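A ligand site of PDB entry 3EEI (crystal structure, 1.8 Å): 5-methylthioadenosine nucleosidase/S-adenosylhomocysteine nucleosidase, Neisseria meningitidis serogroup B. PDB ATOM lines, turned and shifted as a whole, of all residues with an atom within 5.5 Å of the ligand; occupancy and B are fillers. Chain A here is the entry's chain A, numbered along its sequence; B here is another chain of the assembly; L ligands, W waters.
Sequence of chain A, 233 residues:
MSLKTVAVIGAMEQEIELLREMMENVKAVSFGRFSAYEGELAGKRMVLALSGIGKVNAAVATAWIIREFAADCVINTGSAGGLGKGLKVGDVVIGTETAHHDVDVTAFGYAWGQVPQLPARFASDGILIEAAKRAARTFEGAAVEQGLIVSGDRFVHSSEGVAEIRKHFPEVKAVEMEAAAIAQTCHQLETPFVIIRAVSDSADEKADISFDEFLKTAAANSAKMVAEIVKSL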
ATOM      1  N   ALA A  11     -10.003  32.701  -0.334  1.00  0.00           N
ATOM      2  CA  ALA A  11      -9.560  33.136  -1.679  1.00  0.00           C
ATOM      3  C   ALA A  11     -10.386  32.469  -2.793  1.00  0.00           C
ATOM      4  O   ALA A  11     -10.684  33.075  -3.828  1.00  0.00           O
ATOM      5  CB  ALA A  11      -8.061  32.761  -1.877  1.00  0.00           C
ATOM      6  N   MET A  12     -10.697  31.203  -2.574  1.00  0.00           N
ATOM      7  CA  MET A  12     -11.276  30.359  -3.617  1.00  0.00           C
ATOM      8  C   MET A  12     -12.644  29.804  -3.185  1.00  0.00           C
ATOM      9  O   MET A  12     -12.889  29.620  -2.014  1.00  0.00           O
ATOM     10  CB  MET A  12     -10.337  29.191  -3.878  1.00  0.00           C
ATOM     11  CG  MET A  12      -9.000  29.619  -4.451  1.00  0.00           C
ATOM     12  SD  MET A  12      -7.814  28.277  -4.603  1.00  0.00           S
ATOM     13  CE  MET A  12      -8.452  27.458  -6.068  1.00  0.00           C
ATOM     14  N   GLU A  15     -12.887  27.091  -0.751  1.00  0.00           N
ATOM     15  CA  GLU A  15     -12.505  27.459   0.614  1.00  0.00           C
ATOM     16  C   GLU A  15     -13.629  28.110   1.414  1.00  0.00           C
ATOM     17  O   GLU A  15     -13.551  28.173   2.641  1.00  0.00           O
ATOM     18  CB  GLU A  15     -11.254  28.353   0.600  1.00  0.00           C
ATOM     19  CG  GLU A  15     -10.057  27.562   0.072  1.00  0.00           C
ATOM     20  CD  GLU A  15      -8.871  28.447  -0.209  1.00  0.00           C
ATOM     21  OE1 GLU A  15      -9.072  29.611  -0.625  1.00  0.00           O
ATOM     22  OE2 GLU A  15      -7.724  27.957  -0.034  1.00  0.00           O
ATOM     23  N   ILE A  53      -7.593  35.210  -5.614  1.00  0.00           N
ATOM     24  CA  ILE A  53      -6.229  34.819  -5.239  1.00  0.00           C
ATOM     25  C   ILE A  53      -5.259  35.992  -5.203  1.00  0.00           C
ATOM     26  O   ILE A  53      -5.329  36.870  -6.078  1.00  0.00           O
ATOM     27  CB  ILE A  53      -5.733  33.722  -6.207  1.00  0.00           C
ATOM     28  CG1 ILE A  53      -6.535  32.430  -5.898  1.00  0.00           C
ATOM     29  CG2 ILE A  53      -4.210  33.531  -6.125  1.00  0.00           C
ATOM     30  CD1 ILE A  53      -6.598  31.427  -7.060  1.00  0.00           C
ATOM     31  N   GLY A  54      -4.383  36.024  -4.186  1.00  0.00           N
ATOM     32  CA  GLY A  54      -3.236  36.933  -4.158  1.00  0.00           C
ATOM     33  C   GLY A  54      -3.485  38.188  -3.377  1.00  0.00           C
ATOM     34  O   GLY A  54      -4.601  38.412  -2.874  1.00  0.00           O
ATOM     35  N   SER A  79      -6.257  27.147   2.341  1.00  0.00           N
ATOM     36  CA  SER A  79      -5.197  26.164   2.143  1.00  0.00           C
ATOM     37  C   SER A  79      -3.844  26.863   2.134  1.00  0.00           C
ATOM     38  O   SER A  79      -3.780  28.081   1.945  1.00  0.00           O
ATOM     39  CB  SER A  79      -5.411  25.479   0.786  1.00  0.00           C
ATOM     40  OG  SER A  79      -5.338  26.461  -0.262  1.00  0.00           O
ATOM     41  N   ALA A  80      -2.776  26.098   2.295  1.00  0.00           N
ATOM     42  CA  ALA A  80      -1.430  26.683   2.324  1.00  0.00           C
ATOM     43  C   ALA A  80      -0.392  25.590   2.145  1.00  0.00           C
ATOM     44  O   ALA A  80      -0.681  24.379   2.359  1.00  0.00           O
ATOM     45  CB  ALA A  80      -1.213  27.451   3.659  1.00  0.00           C
ATOM     46  N   GLY A  81       0.823  26.005   1.785  1.00  0.00           N
ATOM     47  CA  GLY A  81       1.948  25.087   1.665  1.00  0.00           C
ATOM     48  C   GLY A  81       2.469  24.845   3.066  1.00  0.00           C
ATOM     49  O   GLY A  81       2.766  25.806   3.821  1.00  0.00           O
ATOM     50  N   ARG A 154       3.079  34.584  -5.151  1.00  0.00           N
ATOM     51  CA  ARG A 154       3.511  33.461  -5.964  1.00  0.00           C
ATOM     52  C   ARG A 154       3.097  32.141  -5.360  1.00  0.00           C
ATOM     53  O   ARG A 154       3.031  31.995  -4.137  1.00  0.00           O
ATOM     54  CB  ARG A 154       5.038  33.487  -6.128  1.00  0.00           C
ATOM     55  CG  ARG A 154       5.816  33.109  -4.888  1.00  0.00           C
ATOM     56  CD  ARG A 154       7.345  33.307  -5.126  1.00  0.00           C
ATOM     57  NE  ARG A 154       7.666  34.735  -5.146  1.00  0.00           N
ATOM     58  CZ  ARG A 154       8.898  35.216  -5.051  1.00  0.00           C
ATOM     59  NH1 ARG A 154       9.117  36.532  -5.127  1.00  0.00           N
ATOM     60  NH2 ARG A 154       9.925  34.379  -4.905  1.00  0.00           N
ATOM     61  N   PHE A 155       2.841  31.159  -6.236  1.00  0.00           N
ATOM     62  CA  PHE A 155       2.585  29.827  -5.758  1.00  0.00           C
ATOM     63  C   PHE A 155       3.934  29.149  -5.701  1.00  0.00           C
ATOM     64  O   PHE A 155       4.624  29.024  -6.734  1.00  0.00           O
ATOM     65  CB  PHE A 155       1.698  29.061  -6.762  1.00  0.00           C
ATOM     66  CG  PHE A 155       1.388  27.701  -6.307  1.00  0.00           C
ATOM     67  CD1 PHE A 155       0.375  27.503  -5.386  1.00  0.00           C
ATOM     68  CD2 PHE A 155       2.115  26.608  -6.782  1.00  0.00           C
ATOM     69  CE1 PHE A 155       0.057  26.242  -4.931  1.00  0.00           C
ATOM     70  CE2 PHE A 155       1.820  25.319  -6.335  1.00  0.00           C
ATOM     71  CZ  PHE A 155       0.778  25.132  -5.416  1.00  0.00           C
ATOM     72  N   VAL A 156       4.349  28.750  -4.509  1.00  0.00           N
ATOM     73  CA  VAL A 156       5.683  28.201  -4.328  1.00  0.00           C
ATOM     74  C   VAL A 156       5.690  26.701  -4.590  1.00  0.00           C
ATOM     75  O   VAL A 156       4.913  25.980  -3.985  1.00  0.00           O
ATOM     76  CB  VAL A 156       6.144  28.428  -2.891  1.00  0.00           C
ATOM     77  CG1 VAL A 156       7.567  27.866  -2.679  1.00  0.00           C
ATOM     78  CG2 VAL A 156       6.172  29.937  -2.581  1.00  0.00           C
ATOM     79  N   HIS A 157       6.566  26.255  -5.491  1.00  0.00           N
ATOM     80  CA  HIS A 157       6.588  24.833  -5.860  1.00  0.00           C
ATOM     81  C   HIS A 157       7.997  24.401  -6.245  1.00  0.00           C
ATOM     82  O   HIS A 157       8.240  23.819  -7.329  1.00  0.00           O
ATOM     83  CB  HIS A 157       5.564  24.586  -6.977  1.00  0.00           C
ATOM     84  CG  HIS A 157       5.893  25.282  -8.263  1.00  0.00           C
ATOM     85  ND1 HIS A 157       6.133  24.593  -9.432  1.00  0.00           N
ATOM     86  CD2 HIS A 157       6.037  26.600  -8.575  1.00  0.00           C
ATOM     87  CE1 HIS A 157       6.434  25.434 -10.398  1.00  0.00           C
ATOM     88  NE2 HIS A 157       6.373  26.660  -9.908  1.00  0.00           N
ATOM     89  N   VAL A 175       3.072  28.654   4.017  1.00  0.00           N
ATOM     90  CA  VAL A 175       3.178  29.701   3.003  1.00  0.00           C
ATOM     91  C   VAL A 175       1.945  29.705   2.134  1.00  0.00           C
ATOM     92  O   VAL A 175       1.424  28.631   1.752  1.00  0.00           O
ATOM     93  CB  VAL A 175       4.452  29.577   2.125  1.00  0.00           C
ATOM     94  CG1 VAL A 175       4.586  28.224   1.448  1.00  0.00           C
ATOM     95  CG2 VAL A 175       4.514  30.717   1.100  1.00  0.00           C
ATOM     96  N   GLU A 176       1.461  30.898   1.831  1.00  0.00           N
ATOM     97  CA  GLU A 176       0.326  31.046   0.920  1.00  0.00           C
ATOM     98  C   GLU A 176       0.348  32.447   0.319  1.00  0.00           C
ATOM     99  O   GLU A 176       1.421  33.014   0.190  1.00  0.00           O
ATOM    100  CB  GLU A 176      -0.992  30.634   1.559  1.00  0.00           C
ATOM    101  CG  GLU A 176      -1.192  31.137   2.999  1.00  0.00           C
ATOM    102  CD  GLU A 176      -1.206  32.636   3.005  1.00  0.00           C
ATOM    103  OE1 GLU A 176      -0.128  33.234   3.230  1.00  0.00           O
ATOM    104  OE2 GLU A 176      -2.283  33.222   2.717  1.00  0.00           O
ATOM    105  N   MET A 177      -0.785  32.973  -0.149  1.00  0.00           N
ATOM    106  CA  MET A 177      -0.730  34.152  -1.022  1.00  0.00           C
ATOM    107  C   MET A 177      -1.667  35.279  -0.578  1.00  0.00           C
ATOM    108  O   MET A 177      -1.721  36.314  -1.269  1.00  0.00           O
ATOM    109  CB  MET A 177      -1.117  33.760  -2.470  1.00  0.00           C
ATOM    110  CG  MET A 177      -0.160  32.733  -3.022  1.00  0.00           C
ATOM    111  SD  MET A 177      -0.565  32.150  -4.719  1.00  0.00           S
ATOM    112  CE  MET A 177      -0.698  33.647  -5.633  1.00  0.00           C
ATOM    113  N   GLU A 178      -2.380  35.095   0.533  1.00  0.00           N
ATOM    114  CA  GLU A 178      -3.288  36.181   1.009  1.00  0.00           C
ATOM    115  C   GLU A 178      -3.126  36.665   2.439  1.00  0.00           C
ATOM    116  O   GLU A 178      -3.452  37.835   2.748  1.00  0.00           O
ATOM    117  CB  GLU A 178      -4.727  35.752   0.824  1.00  0.00           C
ATOM    118  CG  GLU A 178      -5.078  35.489  -0.644  1.00  0.00           C
ATOM    119  CD  GLU A 178      -4.889  34.046  -1.041  1.00  0.00           C
ATOM    120  OE1 GLU A 178      -5.034  33.178  -0.152  1.00  0.00           O
ATOM    121  OE2 GLU A 178      -4.657  33.792  -2.234  1.00  0.00           O
ATOM    122  N   ARG A 197      -5.148  28.349   8.437  1.00  0.00           N
ATOM    123  CA  ARG A 197      -4.927  27.718   7.129  1.00  0.00           C
ATOM    124  C   ARG A 197      -4.684  26.248   7.397  1.00  0.00           C
ATOM    125  O   ARG A 197      -4.294  25.885   8.496  1.00  0.00           O
ATOM    126  CB  ARG A 197      -3.706  28.298   6.400  1.00  0.00           C
ATOM    127  CG  ARG A 197      -3.864  29.789   5.973  1.00  0.00           C
ATOM    128  CD  ARG A 197      -4.672  29.848   4.701  1.00  0.00           C
ATOM    129  NE  ARG A 197      -4.823  31.197   4.179  1.00  0.00           N
ATOM    130  CZ  ARG A 197      -5.002  31.477   2.895  1.00  0.00           C
ATOM    131  NH1 ARG A 197      -5.001  30.507   1.979  1.00  0.00           N
ATOM    132  NH2 ARG A 197      -5.170  32.734   2.530  1.00  0.00           N
ATOM    133  N   SER A 200      -2.280  21.863   2.154  1.00  0.00           N
ATOM    134  CA  SER A 200      -2.718  21.183   0.914  1.00  0.00           C
ATOM    135  C   SER A 200      -1.526  20.589   0.118  1.00  0.00           C
ATOM    136  O   SER A 200      -1.704  19.811  -0.855  1.00  0.00           O
ATOM    137  CB  SER A 200      -3.443  22.197   0.030  1.00  0.00           C
ATOM    138  OG  SER A 200      -2.634  23.368  -0.129  1.00  0.00           O
ATOM    139  N   ASP A 201      -0.314  20.933   0.542  1.00  0.00           N
ATOM    140  CA  ASP A 201       0.908  20.601  -0.163  1.00  0.00           C
ATOM    141  C   ASP A 201       2.101  21.058   0.655  1.00  0.00           C
ATOM    142  O   ASP A 201       1.941  21.685   1.733  1.00  0.00           O
ATOM    143  CB  ASP A 201       0.939  21.293  -1.551  1.00  0.00           C
ATOM    144  CG  ASP A 201       0.921  22.809  -1.442  1.00  0.00           C
ATOM    145  OD1 ASP A 201      -0.186  23.371  -1.427  1.00  0.00           O
ATOM    146  OD2 ASP A 201       2.014  23.407  -1.334  1.00  0.00           O
ATOM    147  N   SER A 202       3.289  20.729   0.164  1.00  0.00           N
ATOM    148  CA  SER A 202       4.560  21.111   0.849  1.00  0.00           C
ATOM    149  C   SER A 202       5.353  22.213   0.151  1.00  0.00           C
ATOM    150  O   SER A 202       6.523  22.391   0.471  1.00  0.00           O
ATOM    151  CB  SER A 202       5.461  19.904   1.011  1.00  0.00           C
ATOM    152  OG  SER A 202       4.854  18.977   1.921  1.00  0.00           O
ATOM    153  N   ALA A 203       4.750  22.878  -0.809  1.00  0.00           N
ATOM    154  CA  ALA A 203       5.366  23.982  -1.547  1.00  0.00           C
ATOM    155  C   ALA A 203       6.636  23.561  -2.273  1.00  0.00           C
ATOM    156  O   ALA A 203       7.502  24.409  -2.580  1.00  0.00           O
ATOM    157  CB  ALA A 203       5.703  25.167  -0.572  1.00  0.00           C
ATOM    158  N   ALA A 207       4.127  20.471  -5.493  1.00  0.00           N
ATOM    159  CA  ALA A 207       3.092  21.186  -4.780  1.00  0.00           C
ATOM    160  C   ALA A 207       1.825  21.382  -5.627  1.00  0.00           C
ATOM    161  O   ALA A 207       0.706  21.317  -5.118  1.00  0.00           O
ATOM    162  CB  ALA A 207       3.653  22.570  -4.314  1.00  0.00           C
ATOM    163  N   PHE A 211      -1.660  20.071  -4.426  1.00  0.00           N
ATOM    164  CA  PHE A 211      -2.671  21.082  -4.135  1.00  0.00           C
ATOM    165  C   PHE A 211      -4.094  20.748  -4.614  1.00  0.00           C
ATOM    166  O   PHE A 211      -5.070  20.840  -3.876  1.00  0.00           O
ATOM    167  CB  PHE A 211      -2.245  22.430  -4.712  1.00  0.00           C
ATOM    168  CG  PHE A 211      -3.294  23.486  -4.588  1.00  0.00           C
ATOM    169  CD1 PHE A 211      -3.517  24.101  -3.359  1.00  0.00           C
ATOM    170  CD2 PHE A 211      -4.075  23.847  -5.686  1.00  0.00           C
ATOM    171  CE1 PHE A 211      -4.513  25.056  -3.218  1.00  0.00           C
ATOM    172  CE2 PHE A 211      -5.079  24.823  -5.556  1.00  0.00           C
ATOM    173  CZ  PHE A 211      -5.301  25.433  -4.318  1.00  0.00           C
ATOM    174  N   VAL B 105       2.029  32.485 -10.765  1.00  0.00           N
ATOM    175  CA  VAL B 105       1.225  31.289 -10.563  1.00  0.00           C
ATOM    176  C   VAL B 105       1.390  30.437 -11.844  1.00  0.00           C
ATOM    177  O   VAL B 105       0.444  29.795 -12.316  1.00  0.00           O
ATOM    178  CB  VAL B 105      -0.257  31.645 -10.274  1.00  0.00           C
ATOM    179  CG1 VAL B 105      -1.027  30.418  -9.756  1.00  0.00           C
ATOM    180  CG2 VAL B 105      -0.344  32.733  -9.211  1.00  0.00           C
ATOM    181  N   PHE B 108       0.385  26.704 -12.561  1.00  0.00           N
ATOM    182  CA  PHE B 108      -0.905  26.236 -12.968  1.00  0.00           C
ATOM    183  C   PHE B 108      -1.235  26.730 -14.345  1.00  0.00           C
ATOM    184  O   PHE B 108      -2.425  26.830 -14.720  1.00  0.00           O
ATOM    185  CB  PHE B 108      -1.969  26.687 -11.976  1.00  0.00           C
ATOM    186  CG  PHE B 108      -1.887  26.001 -10.653  1.00  0.00           C
ATOM    187  CD1 PHE B 108      -2.192  24.655 -10.552  1.00  0.00           C
ATOM    188  CD2 PHE B 108      -1.519  26.696  -9.503  1.00  0.00           C
ATOM    189  CE1 PHE B 108      -2.123  23.997  -9.316  1.00  0.00           C
ATOM    190  CE2 PHE B 108      -1.444  26.050  -8.249  1.00  0.00           C
ATOM    191  CZ  PHE B 108      -1.775  24.701  -8.170  1.00  0.00           C
ATOM    192  N   PRO B 116      -4.462  34.733 -11.105  1.00  0.00           N
ATOM    193  CA  PRO B 116      -5.480  33.835 -11.673  1.00  0.00           C
ATOM    194  C   PRO B 116      -6.869  34.468 -11.904  1.00  0.00           C
ATOM    195  O   PRO B 116      -7.375  35.241 -11.103  1.00  0.00           O
ATOM    196  CB  PRO B 116      -5.549  32.683 -10.667  1.00  0.00           C
ATOM    197  CG  PRO B 116      -4.148  32.615 -10.141  1.00  0.00           C
ATOM    198  CD  PRO B 116      -3.687  34.071 -10.043  1.00  0.00           C
HETATM  199  C1  LIG L   1      -4.117  28.333  -6.930  1.00  0.00           C
HETATM  200  S1  LIG L   1      -2.897  29.365  -6.128  1.00  0.00           S
HETATM  201  C2  LIG L   1      -2.860  28.813  -4.455  1.00  0.00           C
HETATM  202  C3  LIG L   1      -4.066  29.202  -3.602  1.00  0.00           C
HETATM  203  N1  LIG L   1      -4.051  28.383  -2.386  1.00  0.00           N
HETATM  204  C4  LIG L   1      -2.760  30.368  -1.882  1.00  0.00           C
HETATM  205  O1  LIG L   1      -3.052  31.279  -0.798  1.00  0.00           O
HETATM  206  C5  LIG L   1      -3.706  30.615  -3.077  1.00  0.00           C
HETATM  207  O2  LIG L   1      -4.889  31.338  -2.694  1.00  0.00           O
HETATM  208  C6  LIG L   1      -3.035  28.918  -1.460  1.00  0.00           C
HETATM  209  C7  LIG L   1      -1.735  28.097  -1.284  1.00  0.00           C
HETATM  210  C8  LIG L   1      -1.743  26.585  -1.144  1.00  0.00           C
HETATM  211  N2  LIG L   1      -0.472  26.081  -1.373  1.00  0.00           N
HETATM  212  C9  LIG L   1       0.368  27.107  -1.747  1.00  0.00           C
HETATM  213  C10 LIG L   1       1.776  27.205  -2.136  1.00  0.00           C
HETATM  214  N3  LIG L   1       2.546  26.103  -2.144  1.00  0.00           N
HETATM  215  N4  LIG L   1       2.312  28.432  -2.434  1.00  0.00           N
HETATM  216  C11 LIG L   1       1.522  29.515  -2.400  1.00  0.00           C
HETATM  217  N5  LIG L   1       0.227  29.530  -2.049  1.00  0.00           N
HETATM  218  C12 LIG L   1      -0.405  28.359  -1.767  1.00  0.00           C
HETATM  219  O   HOH W   1      -5.997  29.718  -0.782  1.00  0.00           O
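An oxygen (O2) of the ligand sits at hydrogen-bond distance from the side-chain carboxylate (OE2) of Glu 178.
The side-chain carboxylate (OD2) of Asp 201 is in salt-bridge range of a nitrogen (N3) of the ligand (2.9 Å).
N of Met 177 is in hydrogen-bond range of O1 of the ligand (2.9 Å).
O of Val 156 lies within hydrogen-bond range of N3 of the ligand (3.0 Å).
OG of Ser 79 is in hydrogen-bond range of N1 of the ligand, at 3.1 Å.
The backbone NH (N) of Gly 81 lies close to a nitrogen (N2) of the ligand, at 3.4 Å.
The guanidinium group of Arg 197 lies within hydrogen-bond range of an oxygen (O1) of the ligand (3.5 Å).
Residues that only touch the ligand: Glu 176 (3.2 Å), Phe 155 (3.3 Å), Arg 154 (3.4 Å), Phe 211 (3.5 Å), Ala 80 (3.5 Å), Ser 200 (3.5 Å), Ala 11 (3.6 Å), Ala 203 (3.6 Å), Phe 108 of chain B (3.8 Å), Ile 53 (3.8 Å), Val 175 (3.96 Å) and Met 12 (3.99 Å).
19 residues have an atom within 4 Å of the ligand: Ala 11, Met 12, Ile 53, Ser 79, Ala 80, Gly 81, Arg 154, Phe 155, Val 156, Val 175, Glu 176, Met 177, Glu 178, Arg 197, Ser 200, Asp 201, Ala 203, Phe 211 and Phe 108 of chain B.
Along chain A the residues within 4 Å of the ligand span positions 11 to 211.
Water W1 lies within hydrogen-bond range of OE2 of Glu 15, O2 of the ligand, NH1 of Arg 197 and OG of Ser 79.
The side-chain carboxylate (OE2) of Glu 176 sits at hydrogen-bond distance from the backbone NH (N) of Glu 178, 2.9 Å away.
The guanidinium group (NH2) of Arg 197 is in salt-bridge range of the side-chain carboxylate (OE1) of Glu 178 (2.7 Å).
The side-chain carboxylate (OD1) of Asp 201 is in hydrogen-bond range of the side-chain hydroxyl (OG) of Ser 200 (2.8 Å).
OD2 of Asp 201 sits at hydrogen-bond distance from N of Ala 203 (2.8 Å).
The guanidinium group (NH2) of Arg 197 lies within salt-bridge range of the side-chain carboxylate (OE2) of Glu 176, at 2.9 Å.
N of Gly 81 sits at hydrogen-bond distance from O of Val 175.
The side-chain carboxylate of Glu 15 lies within hydrogen-bond range of the backbone NH of Ala 11 (3.2 Å).
N of Met 12 sits at hydrogen-bond distance from OE1 of Glu 15 (3.0 Å).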
